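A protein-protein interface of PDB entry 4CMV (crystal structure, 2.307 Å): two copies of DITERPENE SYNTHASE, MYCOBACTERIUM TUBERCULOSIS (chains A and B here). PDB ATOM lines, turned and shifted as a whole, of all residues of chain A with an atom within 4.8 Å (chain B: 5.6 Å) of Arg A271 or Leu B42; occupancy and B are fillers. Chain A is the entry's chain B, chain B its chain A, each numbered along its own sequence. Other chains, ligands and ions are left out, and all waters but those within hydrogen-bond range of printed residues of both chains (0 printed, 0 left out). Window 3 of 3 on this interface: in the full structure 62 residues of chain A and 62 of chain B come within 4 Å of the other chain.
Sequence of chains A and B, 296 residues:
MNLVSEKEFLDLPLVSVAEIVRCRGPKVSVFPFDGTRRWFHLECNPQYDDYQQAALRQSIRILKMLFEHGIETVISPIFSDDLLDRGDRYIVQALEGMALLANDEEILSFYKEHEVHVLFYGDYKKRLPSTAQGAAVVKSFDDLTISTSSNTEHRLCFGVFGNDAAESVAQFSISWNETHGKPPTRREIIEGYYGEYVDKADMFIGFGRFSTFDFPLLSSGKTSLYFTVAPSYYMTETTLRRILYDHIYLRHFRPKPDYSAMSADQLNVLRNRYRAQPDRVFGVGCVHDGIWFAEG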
ATOM      1  N   ALA A 264       2.781 -19.329 -23.972  1.00  0.00           N
ATOM      2  CA  ALA A 264       1.470 -19.413 -23.351  1.00  0.00           C
ATOM      3  C   ALA A 264       0.374 -19.341 -24.404  1.00  0.00           C
ATOM      4  O   ALA A 264      -0.717 -19.868 -24.198  1.00  0.00           O
ATOM      5  CB  ALA A 264       1.287 -18.298 -22.334  1.00  0.00           C
ATOM      6  N   LEU A 267      -0.027 -22.928 -26.164  1.00  0.00           N
ATOM      7  CA  LEU A 267      -0.796 -23.761 -25.258  1.00  0.00           C
ATOM      8  C   LEU A 267      -2.238 -23.282 -25.187  1.00  0.00           C
ATOM      9  O   LEU A 267      -3.148 -24.096 -25.222  1.00  0.00           O
ATOM     10  CB  LEU A 267      -0.185 -23.797 -23.856  1.00  0.00           C
ATOM     11  CG  LEU A 267       1.144 -24.522 -23.586  1.00  0.00           C
ATOM     12  CD1 LEU A 267       1.520 -25.493 -24.712  1.00  0.00           C
ATOM     13  CD2 LEU A 267       2.277 -23.572 -23.259  1.00  0.00           C
ATOM     14  N   ASN A 268      -2.447 -21.971 -25.142  1.00  0.00           N
ATOM     15  CA  ASN A 268      -3.799 -21.434 -25.019  1.00  0.00           C
ATOM     16  C   ASN A 268      -4.670 -21.766 -26.211  1.00  0.00           C
ATOM     17  O   ASN A 268      -5.837 -22.129 -26.062  1.00  0.00           O
ATOM     18  CB  ASN A 268      -3.766 -19.917 -24.849  1.00  0.00           C
ATOM     19  CG  ASN A 268      -3.573 -19.498 -23.413  1.00  0.00           C
ATOM     20  OD1 ASN A 268      -3.805 -20.282 -22.485  1.00  0.00           O
ATOM     21  ND2 ASN A 268      -3.161 -18.250 -23.214  1.00  0.00           N
ATOM     22  N   VAL A 269      -4.097 -21.627 -27.397  1.00  0.00           N
ATOM     23  CA  VAL A 269      -4.805 -21.970 -28.616  1.00  0.00           C
ATOM     24  C   VAL A 269      -5.149 -23.453 -28.621  1.00  0.00           C
ATOM     25  O   VAL A 269      -6.322 -23.812 -28.782  1.00  0.00           O
ATOM     26  CB  VAL A 269      -3.996 -21.598 -29.861  1.00  0.00           C
ATOM     27  CG1 VAL A 269      -4.628 -22.207 -31.089  1.00  0.00           C
ATOM     28  CG2 VAL A 269      -3.927 -20.088 -29.990  1.00  0.00           C
ATOM     29  N   LEU A 270      -4.141 -24.310 -28.437  1.00  0.00           N
ATOM     30  CA  LEU A 270      -4.403 -25.757 -28.383  1.00  0.00           C
ATOM     31  C   LEU A 270      -5.540 -26.107 -27.401  1.00  0.00           C
ATOM     32  O   LEU A 270      -6.517 -26.801 -27.739  1.00  0.00           O
ATOM     33  CB  LEU A 270      -3.133 -26.507 -27.964  1.00  0.00           C
ATOM     34  CG  LEU A 270      -2.055 -26.789 -29.009  1.00  0.00           C
ATOM     35  CD1 LEU A 270      -0.932 -27.623 -28.407  1.00  0.00           C
ATOM     36  CD2 LEU A 270      -2.650 -27.471 -30.220  1.00  0.00           C
ATOM     37  N   ARG A 271      -5.400 -25.564 -26.198  1.00  0.00           N
ATOM     38  CA  ARG A 271      -6.278 -25.801 -25.063  1.00  0.00           C
ATOM     39  C   ARG A 271      -7.723 -25.364 -25.334  1.00  0.00           C
ATOM     40  O   ARG A 271      -8.661 -26.131 -25.096  1.00  0.00           O
ATOM     41  CB  ARG A 271      -5.679 -25.092 -23.836  1.00  0.00           C
ATOM     42  CG  ARG A 271      -6.315 -25.414 -22.498  1.00  0.00           C
ATOM     43  CD  ARG A 271      -5.375 -25.046 -21.336  1.00  0.00           C
ATOM     44  NE  ARG A 271      -4.626 -23.812 -21.559  1.00  0.00           N
ATOM     45  CZ  ARG A 271      -3.355 -23.619 -21.202  1.00  0.00           C
ATOM     46  NH1 ARG A 271      -2.661 -24.585 -20.606  1.00  0.00           N
ATOM     47  NH2 ARG A 271      -2.767 -22.450 -21.444  1.00  0.00           N
ATOM     48  N   ASN A 272      -7.905 -24.155 -25.859  1.00  0.00           N
ATOM     49  CA  ASN A 272      -9.248 -23.674 -26.164  1.00  0.00           C
ATOM     50  C   ASN A 272      -9.855 -24.400 -27.368  1.00  0.00           C
ATOM     51  O   ASN A 272     -11.074 -24.544 -27.459  1.00  0.00           O
ATOM     52  CB  ASN A 272      -9.250 -22.161 -26.403  1.00  0.00           C
ATOM     53  CG  ASN A 272      -8.897 -21.369 -25.146  1.00  0.00           C
ATOM     54  OD1 ASN A 272      -8.998 -21.875 -24.026  1.00  0.00           O
ATOM     55  ND2 ASN A 272      -8.502 -20.114 -25.332  1.00  0.00           N
ATOM     56  N   ARG A 273      -9.010 -24.861 -28.284  1.00  0.00           N
ATOM     57  CA  ARG A 273      -9.488 -25.695 -29.383  1.00  0.00           C
ATOM     58  C   ARG A 273     -10.052 -27.021 -28.838  1.00  0.00           C
ATOM     59  O   ARG A 273     -11.131 -27.473 -29.243  1.00  0.00           O
ATOM     60  CB  ARG A 273      -8.348 -25.946 -30.382  1.00  0.00           C
ATOM     61  CG  ARG A 273      -8.672 -26.850 -31.578  1.00  0.00           C
ATOM     62  CD  ARG A 273      -9.370 -26.129 -32.738  1.00  0.00           C
ATOM     63  NE  ARG A 273      -9.153 -26.814 -34.022  1.00  0.00           N
ATOM     64  CZ  ARG A 273      -9.827 -27.891 -34.438  1.00  0.00           C
ATOM     65  NH1 ARG A 273     -10.777 -28.436 -33.682  1.00  0.00           N
ATOM     66  NH2 ARG A 273      -9.545 -28.436 -35.615  1.00  0.00           N
ATOM     67  N   TYR A 274      -9.344 -27.615 -27.884  1.00  0.00           N
ATOM     68  CA  TYR A 274      -9.752 -28.908 -27.339  1.00  0.00           C
ATOM     69  C   TYR A 274     -10.936 -28.792 -26.385  1.00  0.00           C
ATOM     70  O   TYR A 274     -11.714 -29.728 -26.217  1.00  0.00           O
ATOM     71  CB  TYR A 274      -8.575 -29.567 -26.628  1.00  0.00           C
ATOM     72  CG  TYR A 274      -7.433 -29.879 -27.571  1.00  0.00           C
ATOM     73  CD1 TYR A 274      -7.667 -30.070 -28.925  1.00  0.00           C
ATOM     74  CD2 TYR A 274      -6.128 -29.987 -27.104  1.00  0.00           C
ATOM     75  CE1 TYR A 274      -6.641 -30.359 -29.791  1.00  0.00           C
ATOM     76  CE2 TYR A 274      -5.090 -30.278 -27.963  1.00  0.00           C
ATOM     77  CZ  TYR A 274      -5.349 -30.473 -29.314  1.00  0.00           C
ATOM     78  OH  TYR A 274      -4.310 -30.777 -30.188  1.00  0.00           O
ATOM     79  N   ARG A 275     -11.051 -27.644 -25.739  1.00  0.00           N
ATOM     80  CA  ARG A 275     -12.146 -27.413 -24.811  1.00  0.00           C
ATOM     81  C   ARG A 275     -13.450 -27.040 -25.515  1.00  0.00           C
ATOM     82  O   ARG A 275     -14.525 -27.129 -24.925  1.00  0.00           O
ATOM     83  CB  ARG A 275     -11.757 -26.333 -23.805  1.00  0.00           C
ATOM     84  CG  ARG A 275     -10.866 -26.865 -22.708  1.00  0.00           C
ATOM     85  CD  ARG A 275     -10.291 -25.754 -21.869  1.00  0.00           C
ATOM     86  NE  ARG A 275      -9.476 -26.281 -20.783  1.00  0.00           N
ATOM     87  CZ  ARG A 275      -8.998 -25.539 -19.790  1.00  0.00           C
ATOM     88  NH1 ARG A 275      -9.278 -24.242 -19.739  1.00  0.00           N
ATOM     89  NH2 ARG A 275      -8.256 -26.092 -18.839  1.00  0.00           N
ATOM     90  N   ARG B  37      -0.203 -37.229 -23.205  1.00  0.00           N
ATOM     91  CA  ARG B  37       0.916 -36.366 -22.835  1.00  0.00           C
ATOM     92  C   ARG B  37       0.579 -34.906 -23.118  1.00  0.00           C
ATOM     93  O   ARG B  37       0.817 -34.008 -22.294  1.00  0.00           O
ATOM     94  CB  ARG B  37       2.168 -36.761 -23.614  1.00  0.00           C
ATOM     95  CG  ARG B  37       2.760 -38.115 -23.262  1.00  0.00           C
ATOM     96  CD  ARG B  37       3.906 -38.417 -24.235  1.00  0.00           C
ATOM     97  NE  ARG B  37       4.368 -39.800 -24.178  1.00  0.00           N
ATOM     98  CZ  ARG B  37       3.805 -40.807 -24.838  1.00  0.00           C
ATOM     99  NH1 ARG B  37       2.736 -40.596 -25.602  1.00  0.00           N
ATOM    100  NH2 ARG B  37       4.302 -42.035 -24.725  1.00  0.00           N
ATOM    101  N   ARG B  38       0.010 -34.686 -24.296  1.00  0.00           N
ATOM    102  CA  ARG B  38      -0.462 -33.367 -24.691  1.00  0.00           C
ATOM    103  C   ARG B  38      -1.555 -32.894 -23.730  1.00  0.00           C
ATOM    104  O   ARG B  38      -1.500 -31.772 -23.205  1.00  0.00           O
ATOM    105  CB  ARG B  38      -0.970 -33.404 -26.134  1.00  0.00           C
ATOM    106  CG  ARG B  38      -1.297 -32.063 -26.702  1.00  0.00           C
ATOM    107  CD  ARG B  38      -1.793 -32.182 -28.139  1.00  0.00           C
ATOM    108  NE  ARG B  38      -0.910 -32.987 -28.981  1.00  0.00           N
ATOM    109  CZ  ARG B  38      -1.215 -33.359 -30.223  1.00  0.00           C
ATOM    110  NH1 ARG B  38      -2.374 -32.990 -30.753  1.00  0.00           N
ATOM    111  NH2 ARG B  38      -0.368 -34.090 -30.940  1.00  0.00           N
ATOM    112  N   TRP B  39      -2.518 -33.772 -23.474  1.00  0.00           N
ATOM    113  CA  TRP B  39      -3.579 -33.468 -22.519  1.00  0.00           C
ATOM    114  C   TRP B  39      -2.985 -33.038 -21.179  1.00  0.00           C
ATOM    115  O   TRP B  39      -3.379 -32.013 -20.629  1.00  0.00           O
ATOM    116  CB  TRP B  39      -4.525 -34.669 -22.310  1.00  0.00           C
ATOM    117  CG  TRP B  39      -5.418 -34.447 -21.114  1.00  0.00           C
ATOM    118  CD1 TRP B  39      -6.588 -33.731 -21.075  1.00  0.00           C
ATOM    119  CD2 TRP B  39      -5.175 -34.886 -19.770  1.00  0.00           C
ATOM    120  NE1 TRP B  39      -7.091 -33.711 -19.791  1.00  0.00           N
ATOM    121  CE2 TRP B  39      -6.243 -34.411 -18.973  1.00  0.00           C
ATOM    122  CE3 TRP B  39      -4.165 -35.641 -19.164  1.00  0.00           C
ATOM    123  CZ2 TRP B  39      -6.328 -34.678 -17.608  1.00  0.00           C
ATOM    124  CZ3 TRP B  39      -4.253 -35.902 -17.807  1.00  0.00           C
ATOM    125  CH2 TRP B  39      -5.326 -35.429 -17.049  1.00  0.00           C
ATOM    126  N   PHE B  40      -2.011 -33.802 -20.685  1.00  0.00           N
ATOM    127  CA  PHE B  40      -1.414 -33.581 -19.367  1.00  0.00           C
ATOM    128  C   PHE B  40      -0.694 -32.256 -19.329  1.00  0.00           C
ATOM    129  O   PHE B  40      -0.756 -31.560 -18.320  1.00  0.00           O
ATOM    130  CB  PHE B  40      -0.444 -34.709 -19.010  1.00  0.00           C
ATOM    131  CG  PHE B  40       0.153 -34.589 -17.635  1.00  0.00           C
ATOM    132  CD1 PHE B  40      -0.609 -34.829 -16.499  1.00  0.00           C
ATOM    133  CD2 PHE B  40       1.481 -34.204 -17.477  1.00  0.00           C
ATOM    134  CE1 PHE B  40      -0.062 -34.707 -15.237  1.00  0.00           C
ATOM    135  CE2 PHE B  40       2.038 -34.083 -16.221  1.00  0.00           C
ATOM    136  CZ  PHE B  40       1.266 -34.337 -15.097  1.00  0.00           C
ATOM    137  N   HIS B  41      -0.035 -31.894 -20.431  1.00  0.00           N
ATOM    138  CA  HIS B  41       0.651 -30.597 -20.494  1.00  0.00           C
ATOM    139  C   HIS B  41      -0.269 -29.414 -20.665  1.00  0.00           C
ATOM    140  O   HIS B  41       0.103 -28.287 -20.346  1.00  0.00           O
ATOM    141  CB  HIS B  41       1.669 -30.592 -21.616  1.00  0.00           C
ATOM    142  CG  HIS B  41       2.911 -31.330 -21.263  1.00  0.00           C
ATOM    143  ND1 HIS B  41       2.968 -32.708 -21.222  1.00  0.00           N
ATOM    144  CD2 HIS B  41       4.119 -30.887 -20.855  1.00  0.00           C
ATOM    145  CE1 HIS B  41       4.173 -33.081 -20.840  1.00  0.00           C
ATOM    146  NE2 HIS B  41       4.891 -31.996 -20.615  1.00  0.00           N
ATOM    147  N   LEU B  42      -1.469 -29.656 -21.165  1.00  0.00           N
ATOM    148  CA  LEU B  42      -2.417 -28.566 -21.287  1.00  0.00           C
ATOM    149  C   LEU B  42      -3.292 -28.363 -20.035  1.00  0.00           C
ATOM    150  O   LEU B  42      -3.605 -27.224 -19.699  1.00  0.00           O
ATOM    151  CB  LEU B  42      -3.296 -28.799 -22.516  1.00  0.00           C
ATOM    152  CG  LEU B  42      -2.534 -28.791 -23.841  1.00  0.00           C
ATOM    153  CD1 LEU B  42      -3.476 -29.016 -25.012  1.00  0.00           C
ATOM    154  CD2 LEU B  42      -1.781 -27.480 -23.993  1.00  0.00           C
ATOM    155  N   GLU B  43      -3.662 -29.447 -19.345  1.00  0.00           N
ATOM    156  CA  GLU B  43      -4.718 -29.384 -18.326  1.00  0.00           C
ATOM    157  C   GLU B  43      -4.254 -29.524 -16.873  1.00  0.00           C
ATOM    158  O   GLU B  43      -4.988 -29.161 -15.960  1.00  0.00           O
ATOM    159  CB  GLU B  43      -5.790 -30.456 -18.598  1.00  0.00           C
ATOM    160  CG  GLU B  43      -6.502 -30.270 -19.950  1.00  0.00           C
ATOM    161  CD  GLU B  43      -7.093 -28.871 -20.125  1.00  0.00           C
ATOM    162  OE1 GLU B  43      -7.635 -28.306 -19.149  1.00  0.00           O
ATOM    163  OE2 GLU B  43      -6.957 -28.312 -21.235  1.00  0.00           O
ATOM    164  N   CYS B  44      -3.064 -30.073 -16.660  1.00  0.00           N
ATOM    165  CA  CYS B  44      -2.554 -30.301 -15.313  1.00  0.00           C
ATOM    166  C   CYS B  44      -1.169 -29.624 -15.199  1.00  0.00           C
ATOM    167  O   CYS B  44      -0.727 -28.950 -16.132  1.00  0.00           O
ATOM    168  CB  CYS B  44      -2.536 -31.811 -14.992  1.00  0.00           C
ATOM    169  SG  CYS B  44      -4.227 -32.485 -14.524  1.00  0.00           S
ATOM    170  N   TYR B 234     -10.293 -35.342 -23.329  1.00  0.00           N
ATOM    171  CA  TYR B 234     -11.217 -34.217 -23.454  1.00  0.00           C
ATOM    172  C   TYR B 234     -12.620 -34.707 -23.807  1.00  0.00           C
ATOM    173  O   TYR B 234     -13.554 -33.907 -23.923  1.00  0.00           O
ATOM    174  CB  TYR B 234     -10.743 -33.227 -24.523  1.00  0.00           C
ATOM    175  CG  TYR B 234      -9.575 -32.356 -24.127  1.00  0.00           C
ATOM    176  CD1 TYR B 234      -9.761 -31.216 -23.347  1.00  0.00           C
ATOM    177  CD2 TYR B 234      -8.283 -32.646 -24.574  1.00  0.00           C
ATOM    178  CE1 TYR B 234      -8.693 -30.405 -23.002  1.00  0.00           C
ATOM    179  CE2 TYR B 234      -7.216 -31.847 -24.237  1.00  0.00           C
ATOM    180  CZ  TYR B 234      -7.430 -30.727 -23.458  1.00  0.00           C
ATOM    181  OH  TYR B 234      -6.373 -29.927 -23.120  1.00  0.00           O
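No position is printed for both chains.
Of the 8 pairs that touch across the chains among the printed residues, none has its exchanged pair printed and touching as well.
The side-chain carboxylate of Glu B43 sits at hydrogen-bond distance from the side-chain hydroxyl of Tyr B234, at 2.6 Å.
OD1 of Asn A268 lies within hydrogen-bond range of NH2 of Arg A271 (2.6 Å).
The guanidinium group (NH1) of Arg A271 sits at hydrogen-bond distance from the backbone carbonyl oxygen (O) of Leu B42.
The guanidinium group of Arg B38 sits at hydrogen-bond distance from the side-chain hydroxyl of Tyr A274, 3.0 Å away.
The side-chain carboxylate (OE1) of Glu B43 is in salt-bridge range of the guanidinium group (NE) of Arg A275, at 3.2 Å.
Leu A267 touches Leu B42 (O to CD2, 3.9 Å).
CB of Leu A270 touches CD1 of Leu B42, at 3.9 Å.
CG of Arg A271 touches OE2 of Glu B43, 3.2 Å away.
Tyr A274 touches Leu B42.
Tyr A274 touches Tyr B234.
Of the 9 printed residues of chain B, 4 touch a printed residue of chain A.
Printed residues of chain A that touch a printed residue of chain B: Leu A267, Leu A270, Arg A271, Tyr A274 and Arg A275.
Hydrophobic or aromatic side chains of chain A that line the printed part of chain B: Leu A267, Leu A270 and Tyr A274.
Among the printed residues, Asp or Glu carboxylates within 4 Å of a Lys or Arg side-chain nitrogen of the other chain: Arg A275 with Glu B43 (2.3 Å).
Ala A264 touches none of the printed residues of chain B.
Of the printed residues of chain B, Leu A267 touches Leu B42.
Val A269 touches none of the printed residues of chain B.
Of the printed residues of chain B, Leu A270 touches Leu B42.
Of chain B, only Leu B42 and Glu B43 come within 4 Å of Arg A271.
Printed residues of chain B within 4 Å of Tyr A274: Arg B38 (3.0 Å), Leu B42 (3.5 Å) and Tyr B234 (3.6 Å).
Printed residues of chain B within 4 Å of Arg A275: Glu B43 (2.3 Å).
Printed residues of chain A within 4 Å of Tyr B234: Tyr A274 (3.6 Å).
The nearest residue of chain B that does not touch Arg A271 is Tyr B234 (4.6 Å).
The nearest printed residue of chain B that does not touch Leu A270 is Arg B38 (4.6 Å).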
